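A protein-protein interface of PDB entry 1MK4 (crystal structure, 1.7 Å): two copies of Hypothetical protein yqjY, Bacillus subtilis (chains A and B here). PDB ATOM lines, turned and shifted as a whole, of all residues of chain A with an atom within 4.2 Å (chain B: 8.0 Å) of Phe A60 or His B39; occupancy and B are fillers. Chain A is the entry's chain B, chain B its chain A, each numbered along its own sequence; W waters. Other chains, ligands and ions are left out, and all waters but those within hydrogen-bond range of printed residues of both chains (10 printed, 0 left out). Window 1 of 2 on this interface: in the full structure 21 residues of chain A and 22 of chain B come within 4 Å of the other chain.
OG of Ser A64 is in hydrogen-bond range of O of Glu B38, 3.2 Å away.
A ring nitrogen (ND1) of His B39 is in hydrogen-bond range of the side-chain hydroxyl (OG) of Ser A62, 2.8 Å away.
The backbone NH (N) of Gln A63 is in hydrogen-bond range of the backbone carbonyl oxygen (O) of His B39 (2.9 Å).
The backbone carbonyl oxygen of His B39 is in hydrogen-bond range of the backbone NH of Ser A64 (3.0 Å).
OG of Ser A64 lies within hydrogen-bond range of N of Gln B41, at 3.4 Å.
The backbone carbonyl oxygen (O) of Gln B61 lies within hydrogen-bond range of the side-chain amide nitrogen (NE2) of Gln A63.
NE2 of Gln B63 sits at hydrogen-bond distance from O of Gln A61 (2.7 Å).
NE2 of Gln B63 lies close to NE2 of Gln A63 (3.3 Å).
The side-chain hydroxyl of Ser B9 is in hydrogen-bond range of the side-chain carboxylate of Glu B38, 2.7 Å away.
O of Phe B37 lies within hydrogen-bond range of NE2 of Gln B41 (2.8 Å).
The backbone carbonyl oxygen of Phe B40 lies within hydrogen-bond range of the side-chain hydroxyl of Ser B44 (2.9 Å).
The side-chain amide oxygen of Gln B61 lies within hydrogen-bond range of the guanidinium group of Arg B100, at 2.8 Å.
The backbone carbonyl oxygen (O) of Phe A60 is in hydrogen-bond range of the backbone NH (N) of Tyr A70 (2.8 Å).
Among the printed residues, pairs that only touch across the chains: Phe A40 with Gln B63, Tyr A70 with His B39, Ser A64 with Phe B40, Gln A63 with Arg B100, Ser A64 with Asp B42, Phe A60 with Gln B63, Gln A63 with Phe B60, Gln A63 with Phe B40, Phe A60 with Phe B40, Phe A40 with Phe B60, Phe A40 with Phe B40 and Phe A60 with His B39.
No residue of chain B comes within 4 Å of Gly A59.
Of the printed residues of chain B, Phe A60 touches His B39, Phe B40 and Gln B63.
Of the printed residues of chain B, Ser A62 touches His B39 (2.8 Å).
Of the printed residues of chain A, Glu B38 touches Ser A64 (3.2 Å).
Printed residues of chain A within 4 Å of Phe B60: Phe A40 and Gln A63.
The nearest printed residue of chain A that does not touch His B39 is Gln A61 (5.5 Å).
The nearest printed residue of chain A that does not touch Arg B100 is Ser A64 (6.2 Å).
Of the 11 printed residues of chain A, 7 touch a printed residue of chain B.
Printed residues of chain A that touch a printed residue of chain B: Phe A40, Phe A60, Gln A61, Ser A62, Gln A63, Ser A64 and Tyr A70.
Hydrophobic or aromatic side chains of chain A that line the printed part of chain B: Phe A40, Phe A60 and Tyr A70.
Printed residues of chain B that touch a printed residue of chain A: Glu B38, His B39, Phe B40, Gln B41, Asp B42, Phe B60, Gln B61, Gln B63 and Arg B100.
Among the printed residues, no Asp or Glu carboxylate lies within 4 Å of a Lys or Arg side-chain nitrogen of the other chain.
Phe A40 touches Phe B60, and with the chains exchanged Phe A60 touches Phe B40.
Phe A40 touches Gln B63, and with the chains exchanged Gln A63 touches Phe B40.
Phe A60 touches Gln B63, and with the chains exchanged Gln A63 touches Phe B60.
Gln B63 touches its own counterpart, Gln A63.
Positions printed for both chains: 40, 43, 59, 60, 61 and 63.
Water W9 lies within hydrogen-bond range of OD2 of Asp B42 (2.7 Å), O of Gln A63 (2.7 Å) and NH1 of Arg B100 (2.8 Å).
Water W5 bridges O of Gln A63 and NH2 of Arg B100.
Water W7 bridges the backbone carbonyl oxygen of Ser A64 and the side-chain carboxylate of Asp B42.
Water W6 lies within hydrogen-bond range of the backbone NH of Asp B42 (2.9 Å) and the backbone NH of Ser A64 (3.5 Å).
Water W1 bridges NE2 of Gln B63 and OE1 of Gln A61.
Water W4 bridges OD2 of Asp B42 (3.4 Å) and O of Ser A64 (3.4 Å).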
ATOM      1  N   PHE A  40      -2.137  -4.513 -10.280  1.00  0.00           N
ATOM      2  CA  PHE A  40      -3.402  -5.109 -10.700  1.00  0.00           C
ATOM      3  C   PHE A  40      -3.185  -5.946 -11.952  1.00  0.00           C
ATOM      4  O   PHE A  40      -4.025  -5.975 -12.846  1.00  0.00           O
ATOM      5  CB  PHE A  40      -4.416  -3.990 -10.962  1.00  0.00           C
ATOM      6  CG  PHE A  40      -4.610  -3.073  -9.784  1.00  0.00           C
ATOM      7  CD1 PHE A  40      -5.262  -3.522  -8.642  1.00  0.00           C
ATOM      8  CD2 PHE A  40      -4.105  -1.778  -9.801  1.00  0.00           C
ATOM      9  CE1 PHE A  40      -5.406  -2.696  -7.528  1.00  0.00           C
ATOM     10  CE2 PHE A  40      -4.242  -0.941  -8.693  1.00  0.00           C
ATOM     11  CZ  PHE A  40      -4.893  -1.403  -7.554  1.00  0.00           C
ATOM     12  N   THR A  43      -5.683  -8.884 -13.394  1.00  0.00           N
ATOM     13  CA  THR A  43      -6.953  -8.478 -13.982  1.00  0.00           C
ATOM     14  C   THR A  43      -6.763  -7.385 -15.026  1.00  0.00           C
ATOM     15  O   THR A  43      -7.679  -6.625 -15.307  1.00  0.00           O
ATOM     16  CB  THR A  43      -7.960  -7.989 -12.909  1.00  0.00           C
ATOM     17  OG1 THR A  43      -7.385  -6.916 -12.160  1.00  0.00           O
ATOM     18  CG2 THR A  43      -8.326  -9.129 -11.964  1.00  0.00           C
ATOM     19  N   GLY A  59      -7.834  -3.088 -15.228  1.00  0.00           N
ATOM     20  CA  GLY A  59      -8.966  -3.133 -14.324  1.00  0.00           C
ATOM     21  C   GLY A  59      -8.593  -3.794 -13.014  1.00  0.00           C
ATOM     22  O   GLY A  59      -7.477  -4.300 -12.857  1.00  0.00           O
ATOM     23  N   PHE A  60      -9.524  -3.797 -12.070  1.00  0.00           N
ATOM     24  CA  PHE A  60      -9.248  -4.396 -10.774  1.00  0.00           C
ATOM     25  C   PHE A  60     -10.521  -4.732 -10.024  1.00  0.00           C
ATOM     26  O   PHE A  60     -11.616  -4.358 -10.437  1.00  0.00           O
ATOM     27  CB  PHE A  60      -8.377  -3.439  -9.937  1.00  0.00           C
ATOM     28  CG  PHE A  60      -8.977  -2.064  -9.742  1.00  0.00           C
ATOM     29  CD1 PHE A  60      -9.999  -1.849  -8.815  1.00  0.00           C
ATOM     30  CD2 PHE A  60      -8.521  -0.984 -10.495  1.00  0.00           C
ATOM     31  CE1 PHE A  60     -10.562  -0.569  -8.645  1.00  0.00           C
ATOM     32  CE2 PHE A  60      -9.074   0.298 -10.335  1.00  0.00           C
ATOM     33  CZ  PHE A  60     -10.096   0.503  -9.408  1.00  0.00           C
ATOM     34  N   GLN A  61     -10.377  -5.467  -8.929  1.00  0.00           N
ATOM     35  CA  GLN A  61     -11.518  -5.802  -8.099  1.00  0.00           C
ATOM     36  C   GLN A  61     -11.617  -4.711  -7.041  1.00  0.00           C
ATOM     37  O   GLN A  61     -10.605  -4.310  -6.463  1.00  0.00           O
ATOM     38  CB  GLN A  61     -11.323  -7.162  -7.419  1.00  0.00           C
ATOM     39  CG  GLN A  61     -12.399  -7.474  -6.387  1.00  0.00           C
ATOM     40  CD  GLN A  61     -12.293  -8.877  -5.836  1.00  0.00           C
ATOM     41  OE1 GLN A  61     -11.214  -9.482  -5.834  1.00  0.00           O
ATOM     42  NE2 GLN A  61     -13.411  -9.404  -5.350  1.00  0.00           N
ATOM     43  N   SER A  62     -12.822  -4.205  -6.805  1.00  0.00           N
ATOM     44  CA  SER A  62     -12.995  -3.180  -5.785  1.00  0.00           C
ATOM     45  C   SER A  62     -12.586  -3.771  -4.448  1.00  0.00           C
ATOM     46  O   SER A  62     -12.884  -4.928  -4.158  1.00  0.00           O
ATOM     47  CB  SER A  62     -14.451  -2.735  -5.697  1.00  0.00           C
ATOM     48  OG  SER A  62     -14.622  -1.818  -4.622  1.00  0.00           O
ATOM     49  N   GLN A  63     -11.911  -2.980  -3.622  1.00  0.00           N
ATOM     50  CA  GLN A  63     -11.506  -3.477  -2.317  1.00  0.00           C
ATOM     51  C   GLN A  63     -12.541  -3.196  -1.227  1.00  0.00           C
ATOM     52  O   GLN A  63     -12.773  -4.040  -0.358  1.00  0.00           O
ATOM     53  CB  GLN A  63     -10.116  -2.933  -1.958  1.00  0.00           C
ATOM     54  CG  GLN A  63      -9.046  -3.933  -2.362  1.00  0.00           C
ATOM     55  CD  GLN A  63      -7.627  -3.417  -2.287  1.00  0.00           C
ATOM     56  OE1 GLN A  63      -7.244  -2.685  -1.353  1.00  0.00           O
ATOM     57  NE2 GLN A  63      -6.819  -3.825  -3.262  1.00  0.00           N
ATOM     58  N   SER A  64     -13.201  -2.042  -1.283  1.00  0.00           N
ATOM     59  CA  SER A  64     -14.218  -1.742  -0.274  1.00  0.00           C
ATOM     60  C   SER A  64     -15.611  -2.278  -0.645  1.00  0.00           C
ATOM     61  O   SER A  64     -16.517  -2.311   0.190  1.00  0.00           O
ATOM     62  CB  SER A  64     -14.261  -0.233   0.016  1.00  0.00           C
ATOM     63  OG  SER A  64     -14.160   0.540  -1.161  1.00  0.00           O
ATOM     64  N   ALA A  69     -16.327  -5.185  -9.742  1.00  0.00           N
ATOM     65  CA  ALA A  69     -15.074  -5.147 -10.492  1.00  0.00           C
ATOM     66  C   ALA A  69     -15.101  -3.791 -11.200  1.00  0.00           C
ATOM     67  O   ALA A  69     -16.176  -3.283 -11.519  1.00  0.00           O
ATOM     68  CB  ALA A  69     -15.022  -6.277 -11.517  1.00  0.00           C
ATOM     69  N   TYR A  70     -13.934  -3.207 -11.443  1.00  0.00           N
ATOM     70  CA  TYR A  70     -13.867  -1.897 -12.087  1.00  0.00           C
ATOM     71  C   TYR A  70     -12.873  -1.862 -13.234  1.00  0.00           C
ATOM     72  O   TYR A  70     -11.732  -2.299 -13.090  1.00  0.00           O
ATOM     73  CB  TYR A  70     -13.487  -0.835 -11.047  1.00  0.00           C
ATOM     74  CG  TYR A  70     -13.460   0.593 -11.553  1.00  0.00           C
ATOM     75  CD1 TYR A  70     -12.285   1.161 -12.055  1.00  0.00           C
ATOM     76  CD2 TYR A  70     -14.613   1.383 -11.517  1.00  0.00           C
ATOM     77  CE1 TYR A  70     -12.260   2.488 -12.508  1.00  0.00           C
ATOM     78  CE2 TYR A  70     -14.598   2.704 -11.966  1.00  0.00           C
ATOM     79  CZ  TYR A  70     -13.420   3.247 -12.459  1.00  0.00           C
ATOM     80  OH  TYR A  70     -13.412   4.552 -12.897  1.00  0.00           O
ATOM     81  N   PHE A  93     -11.666 -10.337 -19.010  1.00  0.00           N
ATOM     82  CA  PHE A  93     -11.680  -9.623 -17.736  1.00  0.00           C
ATOM     83  C   PHE A  93     -12.836 -10.126 -16.868  1.00  0.00           C
ATOM     84  O   PHE A  93     -12.650 -10.426 -15.690  1.00  0.00           O
ATOM     85  CB  PHE A  93     -11.849  -8.118 -17.965  1.00  0.00           C
ATOM     86  CG  PHE A  93     -11.964  -7.316 -16.692  1.00  0.00           C
ATOM     87  CD1 PHE A  93     -10.830  -6.998 -15.946  1.00  0.00           C
ATOM     88  CD2 PHE A  93     -13.208  -6.893 -16.233  1.00  0.00           C
ATOM     89  CE1 PHE A  93     -10.936  -6.268 -14.761  1.00  0.00           C
ATOM     90  CE2 PHE A  93     -13.329  -6.164 -15.048  1.00  0.00           C
ATOM     91  CZ  PHE A  93     -12.192  -5.850 -14.311  1.00  0.00           C
ATOM     92  N   ILE B   7     -12.179   6.848   4.699  1.00  0.00           N
ATOM     93  CA  ILE B   7     -12.829   7.814   3.821  1.00  0.00           C
ATOM     94  C   ILE B   7     -14.104   7.265   3.195  1.00  0.00           C
ATOM     95  O   ILE B   7     -14.342   6.055   3.195  1.00  0.00           O
ATOM     96  CB  ILE B   7     -11.896   8.260   2.686  1.00  0.00           C
ATOM     97  CG1 ILE B   7     -11.588   7.074   1.772  1.00  0.00           C
ATOM     98  CG2 ILE B   7     -10.621   8.849   3.264  1.00  0.00           C
ATOM     99  CD1 ILE B   7     -10.878   7.465   0.493  1.00  0.00           C
ATOM    100  N   SER B   9     -17.115   8.204  -0.180  1.00  0.00           N
ATOM    101  CA  SER B   9     -17.218   8.883  -1.461  1.00  0.00           C
ATOM    102  C   SER B   9     -17.520  10.364  -1.286  1.00  0.00           C
ATOM    103  O   SER B   9     -17.027  11.198  -2.046  1.00  0.00           O
ATOM    104  CB  SER B   9     -18.306   8.233  -2.319  1.00  0.00           C
ATOM    105  OG  SER B   9     -18.324   8.807  -3.617  1.00  0.00           O
ATOM    106  N   PRO B  33      -8.042  10.755  -8.766  1.00  0.00           N
ATOM    107  CA  PRO B  33      -9.298  10.304  -9.377  1.00  0.00           C
ATOM    108  C   PRO B  33     -10.296   9.832  -8.320  1.00  0.00           C
ATOM    109  O   PRO B  33      -9.913   9.302  -7.278  1.00  0.00           O
ATOM    110  CB  PRO B  33      -8.851   9.160 -10.290  1.00  0.00           C
ATOM    111  CG  PRO B  33      -7.434   9.524 -10.629  1.00  0.00           C
ATOM    112  CD  PRO B  33      -6.894  10.009  -9.310  1.00  0.00           C
ATOM    113  N   ARG B  34     -11.578  10.018  -8.611  1.00  0.00           N
ATOM    114  CA  ARG B  34     -12.654   9.625  -7.713  1.00  0.00           C
ATOM    115  C   ARG B  34     -12.617   8.129  -7.378  1.00  0.00           C
ATOM    116  O   ARG B  34     -13.053   7.712  -6.307  1.00  0.00           O
ATOM    117  CB  ARG B  34     -13.997   9.979  -8.367  1.00  0.00           C
ATOM    118  CG  ARG B  34     -15.224   9.770  -7.502  1.00  0.00           C
ATOM    119  CD  ARG B  34     -15.142  10.568  -6.221  1.00  0.00           C
ATOM    120  NE  ARG B  34     -16.420  10.619  -5.519  1.00  0.00           N
ATOM    121  CZ  ARG B  34     -17.362  11.536  -5.728  1.00  0.00           C
ATOM    122  NH1 ARG B  34     -17.185  12.495  -6.627  1.00  0.00           N
ATOM    123  NH2 ARG B  34     -18.482  11.502  -5.021  1.00  0.00           N
ATOM    124  N   LEU B  35     -12.091   7.328  -8.297  1.00  0.00           N
ATOM    125  CA  LEU B  35     -12.034   5.879  -8.109  1.00  0.00           C
ATOM    126  C   LEU B  35     -11.412   5.443  -6.779  1.00  0.00           C
ATOM    127  O   LEU B  35     -11.786   4.411  -6.221  1.00  0.00           O
ATOM    128  CB  LEU B  35     -11.283   5.236  -9.283  1.00  0.00           C
ATOM    129  CG  LEU B  35      -9.771   5.445  -9.392  1.00  0.00           C
ATOM    130  CD1 LEU B  35      -9.048   4.368  -8.590  1.00  0.00           C
ATOM    131  CD2 LEU B  35      -9.350   5.386 -10.854  1.00  0.00           C
ATOM    132  N   PHE B  36     -10.463   6.218  -6.267  1.00  0.00           N
ATOM    133  CA  PHE B  36      -9.839   5.861  -4.994  1.00  0.00           C
ATOM    134  C   PHE B  36     -10.808   6.004  -3.820  1.00  0.00           C
ATOM    135  O   PHE B  36     -10.799   5.190  -2.891  1.00  0.00           O
ATOM    136  CB  PHE B  36      -8.598   6.722  -4.764  1.00  0.00           C
ATOM    137  CG  PHE B  36      -7.450   6.363  -5.654  1.00  0.00           C
ATOM    138  CD1 PHE B  36      -6.703   5.214  -5.413  1.00  0.00           C
ATOM    139  CD2 PHE B  36      -7.134   7.149  -6.753  1.00  0.00           C
ATOM    140  CE1 PHE B  36      -5.654   4.854  -6.259  1.00  0.00           C
ATOM    141  CE2 PHE B  36      -6.093   6.801  -7.605  1.00  0.00           C
ATOM    142  CZ  PHE B  36      -5.349   5.647  -7.357  1.00  0.00           C
ATOM    143  N   PHE B  37     -11.655   7.027  -3.876  1.00  0.00           N
ATOM    144  CA  PHE B  37     -12.629   7.284  -2.822  1.00  0.00           C
ATOM    145  C   PHE B  37     -13.806   6.325  -2.866  1.00  0.00           C
ATOM    146  O   PHE B  37     -14.592   6.240  -1.924  1.00  0.00           O
ATOM    147  CB  PHE B  37     -13.154   8.721  -2.932  1.00  0.00           C
ATOM    148  CG  PHE B  37     -12.116   9.765  -2.658  1.00  0.00           C
ATOM    149  CD1 PHE B  37     -11.098  10.012  -3.570  1.00  0.00           C
ATOM    150  CD2 PHE B  37     -12.154  10.502  -1.477  1.00  0.00           C
ATOM    151  CE1 PHE B  37     -10.127  10.980  -3.313  1.00  0.00           C
ATOM    152  CE2 PHE B  37     -11.188  11.472  -1.211  1.00  0.00           C
ATOM    153  CZ  PHE B  37     -10.176  11.710  -2.129  1.00  0.00           C
ATOM    154  N   GLU B  38     -13.932   5.600  -3.969  1.00  0.00           N
ATOM    155  CA  GLU B  38     -15.026   4.665  -4.115  1.00  0.00           C
ATOM    156  C   GLU B  38     -14.616   3.215  -3.910  1.00  0.00           C
ATOM    157  O   GLU B  38     -15.406   2.418  -3.415  1.00  0.00           O
ATOM    158  CB  GLU B  38     -15.653   4.823  -5.507  1.00  0.00           C
ATOM    159  CG  GLU B  38     -16.311   6.179  -5.737  1.00  0.00           C
ATOM    160  CD  GLU B  38     -17.688   6.279  -5.095  1.00  0.00           C
ATOM    161  OE1 GLU B  38     -17.911   5.641  -4.042  1.00  0.00           O
ATOM    162  OE2 GLU B  38     -18.550   7.004  -5.642  1.00  0.00           O
ATOM    163  N   HIS B  39     -13.376   2.880  -4.249  1.00  0.00           N
ATOM    164  CA  HIS B  39     -12.949   1.490  -4.174  1.00  0.00           C
ATOM    165  C   HIS B  39     -11.869   1.071  -3.197  1.00  0.00           C
ATOM    166  O   HIS B  39     -11.628  -0.124  -3.028  1.00  0.00           O
ATOM    167  CB  HIS B  39     -12.559   1.036  -5.582  1.00  0.00           C
ATOM    168  CG  HIS B  39     -13.689   1.131  -6.555  1.00  0.00           C
ATOM    169  ND1 HIS B  39     -14.826   0.360  -6.439  1.00  0.00           N
ATOM    170  CD2 HIS B  39     -13.902   1.965  -7.600  1.00  0.00           C
ATOM    171  CE1 HIS B  39     -15.694   0.718  -7.367  1.00  0.00           C
ATOM    172  NE2 HIS B  39     -15.158   1.690  -8.085  1.00  0.00           N
ATOM    173  N   PHE B  40     -11.229   2.034  -2.545  1.00  0.00           N
ATOM    174  CA  PHE B  40     -10.169   1.704  -1.604  1.00  0.00           C
ATOM    175  C   PHE B  40     -10.388   2.431  -0.283  1.00  0.00           C
ATOM    176  O   PHE B  40      -9.436   2.874   0.364  1.00  0.00           O
ATOM    177  CB  PHE B  40      -8.820   2.084  -2.220  1.00  0.00           C
ATOM    178  CG  PHE B  40      -8.540   1.390  -3.529  1.00  0.00           C
ATOM    179  CD1 PHE B  40      -8.322   0.017  -3.565  1.00  0.00           C
ATOM    180  CD2 PHE B  40      -8.530   2.103  -4.724  1.00  0.00           C
ATOM    181  CE1 PHE B  40      -8.100  -0.642  -4.780  1.00  0.00           C
ATOM    182  CE2 PHE B  40      -8.309   1.451  -5.944  1.00  0.00           C
ATOM    183  CZ  PHE B  40      -8.096   0.076  -5.968  1.00  0.00           C
ATOM    184  N   GLN B  41     -11.655   2.538   0.105  1.00  0.00           N
ATOM    185  CA  GLN B  41     -12.057   3.233   1.331  1.00  0.00           C
ATOM    186  C   GLN B  41     -11.517   2.696   2.649  1.00  0.00           C
ATOM    187  O   GLN B  41     -11.143   3.479   3.533  1.00  0.00           O
ATOM    188  CB  GLN B  41     -13.584   3.262   1.428  1.00  0.00           C
ATOM    189  CG  GLN B  41     -14.286   3.818   0.215  1.00  0.00           C
ATOM    190  CD  GLN B  41     -15.778   3.911   0.435  1.00  0.00           C
ATOM    191  OE1 GLN B  41     -16.331   3.212   1.283  1.00  0.00           O
ATOM    192  NE2 GLN B  41     -16.441   4.771  -0.330  1.00  0.00           N
ATOM    193  N   ASP B  42     -11.486   1.376   2.796  1.00  0.00           N
ATOM    194  CA  ASP B  42     -11.037   0.762   4.041  1.00  0.00           C
ATOM    195  C   ASP B  42      -9.563   0.895   4.356  1.00  0.00           C
ATOM    196  O   ASP B  42      -9.139   0.583   5.467  1.00  0.00           O
ATOM    197  CB  ASP B  42     -11.440  -0.714   4.071  1.00  0.00           C
ATOM    198  CG  ASP B  42     -12.932  -0.899   3.938  1.00  0.00           C
ATOM    199  OD1 ASP B  42     -13.683  -0.105   4.548  1.00  0.00           O
ATOM    200  OD2 ASP B  42     -13.359  -1.837   3.232  1.00  0.00           O
ATOM    201  N   THR B  43      -8.778   1.352   3.386  1.00  0.00           N
ATOM    202  CA  THR B  43      -7.348   1.534   3.610  1.00  0.00           C
ATOM    203  C   THR B  43      -6.928   2.966   3.278  1.00  0.00           C
ATOM    204  O   THR B  43      -5.764   3.238   2.981  1.00  0.00           O
ATOM    205  CB  THR B  43      -6.521   0.539   2.780  1.00  0.00           C
ATOM    206  OG1 THR B  43      -6.864   0.666   1.402  1.00  0.00           O
ATOM    207  CG2 THR B  43      -6.800  -0.887   3.230  1.00  0.00           C
ATOM    208  N   SER B  44      -7.896   3.876   3.319  1.00  0.00           N
ATOM    209  CA  SER B  44      -7.653   5.297   3.063  1.00  0.00           C
ATOM    210  C   SER B  44      -8.264   6.024   4.253  1.00  0.00           C
ATOM    211  O   SER B  44      -9.354   5.669   4.712  1.00  0.00           O
ATOM    212  CB  SER B  44      -8.294   5.721   1.743  1.00  0.00           C
ATOM    213  OG  SER B  44      -7.623   5.061   0.676  1.00  0.00           O
ATOM    214  N   GLY B  59      -4.469   4.807   0.051  1.00  0.00           N
ATOM    215  CA  GLY B  59      -3.632   3.647  -0.187  1.00  0.00           C
ATOM    216  C   GLY B  59      -4.479   2.415  -0.428  1.00  0.00           C
ATOM    217  O   GLY B  59      -5.707   2.469  -0.328  1.00  0.00           O
ATOM    218  N   PHE B  60      -3.831   1.296  -0.731  1.00  0.00           N
ATOM    219  CA  PHE B  60      -4.565   0.067  -0.998  1.00  0.00           C
ATOM    220  C   PHE B  60      -3.668  -1.154  -0.861  1.00  0.00           C
ATOM    221  O   PHE B  60      -2.449  -1.039  -0.699  1.00  0.00           O
ATOM    222  CB  PHE B  60      -5.163   0.121  -2.420  1.00  0.00           C
ATOM    223  CG  PHE B  60      -4.146   0.381  -3.510  1.00  0.00           C
ATOM    224  CD1 PHE B  60      -3.340  -0.648  -4.001  1.00  0.00           C
ATOM    225  CD2 PHE B  60      -3.975   1.664  -4.026  1.00  0.00           C
ATOM    226  CE1 PHE B  60      -2.376  -0.405  -4.992  1.00  0.00           C
ATOM    227  CE2 PHE B  60      -3.017   1.923  -5.015  1.00  0.00           C
ATOM    228  CZ  PHE B  60      -2.214   0.882  -5.499  1.00  0.00           C
ATOM    229  N   GLN B  61      -4.276  -2.331  -0.909  1.00  0.00           N
ATOM    230  CA  GLN B  61      -3.506  -3.558  -0.848  1.00  0.00           C
ATOM    231  C   GLN B  61      -3.249  -3.966  -2.298  1.00  0.00           C
ATOM    232  O   GLN B  61      -4.137  -3.865  -3.146  1.00  0.00           O
ATOM    233  CB  GLN B  61      -4.290  -4.659  -0.121  1.00  0.00           C
ATOM    234  CG  GLN B  61      -3.627  -6.033  -0.187  1.00  0.00           C
ATOM    235  CD  GLN B  61      -4.372  -7.085   0.620  1.00  0.00           C
ATOM    236  OE1 GLN B  61      -5.567  -6.956   0.881  1.00  0.00           O
ATOM    237  NE2 GLN B  61      -3.671  -8.142   1.005  1.00  0.00           N
ATOM    238  N   GLN B  63      -3.061  -6.164  -5.493  1.00  0.00           N
ATOM    239  CA  GLN B  63      -3.881  -7.321  -5.842  1.00  0.00           C
ATOM    240  C   GLN B  63      -3.041  -8.431  -6.451  1.00  0.00           C
ATOM    241  O   GLN B  63      -3.270  -9.607  -6.165  1.00  0.00           O
ATOM    242  CB  GLN B  63      -5.019  -6.926  -6.795  1.00  0.00           C
ATOM    243  CG  GLN B  63      -5.865  -5.795  -6.240  1.00  0.00           C
ATOM    244  CD  GLN B  63      -7.320  -5.823  -6.680  1.00  0.00           C
ATOM    245  OE1 GLN B  63      -7.662  -6.277  -7.791  1.00  0.00           O
ATOM    246  NE2 GLN B  63      -8.194  -5.308  -5.810  1.00  0.00           N
ATOM    247  N   ARG B 100      -4.860  -7.489   6.677  1.00  0.00           N
ATOM    248  CA  ARG B 100      -5.256  -7.963   5.353  1.00  0.00           C
ATOM    249  C   ARG B 100      -4.213  -8.934   4.809  1.00  0.00           C
ATOM    250  O   ARG B 100      -4.328  -9.400   3.673  1.00  0.00           O
ATOM    251  CB  ARG B 100      -5.404  -6.794   4.370  1.00  0.00           C
ATOM    252  CG  ARG B 100      -6.483  -5.782   4.725  1.00  0.00           C
ATOM    253  CD  ARG B 100      -6.533  -4.665   3.686  1.00  0.00           C
ATOM    254  NE  ARG B 100      -6.998  -5.153   2.390  1.00  0.00           N
ATOM    255  CZ  ARG B 100      -8.260  -5.087   1.976  1.00  0.00           C
ATOM    256  NH1 ARG B 100      -9.190  -4.543   2.753  1.00  0.00           N
ATOM    257  NH2 ARG B 100      -8.595  -5.582   0.790  1.00  0.00           N
HETATM  258  O   HOH W   1      -8.858  -7.847  -4.060  1.00  0.00           O
HETATM  259  O   HOH W   2      -7.452  -6.849  -2.017  1.00  0.00           O
HETATM  260  O   HOH W   3      -6.306  -7.343  -9.662  1.00  0.00           O
HETATM  261  O   HOH W   4     -15.557  -4.324   2.751  1.00  0.00           O
HETATM  262  O   HOH W   5     -11.378  -6.329   0.035  1.00  0.00           O
HETATM  263  O   HOH W   6     -11.019  -0.906   1.139  1.00  0.00           O
HETATM  264  O   HOH W   7     -16.095  -1.712   2.838  1.00  0.00           O
HETATM  265  O   HOH W   8     -16.844   0.959  -1.400  1.00  0.00           O
HETATM  266  O   HOH W   9     -11.753  -3.677   2.147  1.00  0.00           O
HETATM  267  O   HOH W  10      -8.542  -1.081   0.195  1.00  0.00           O
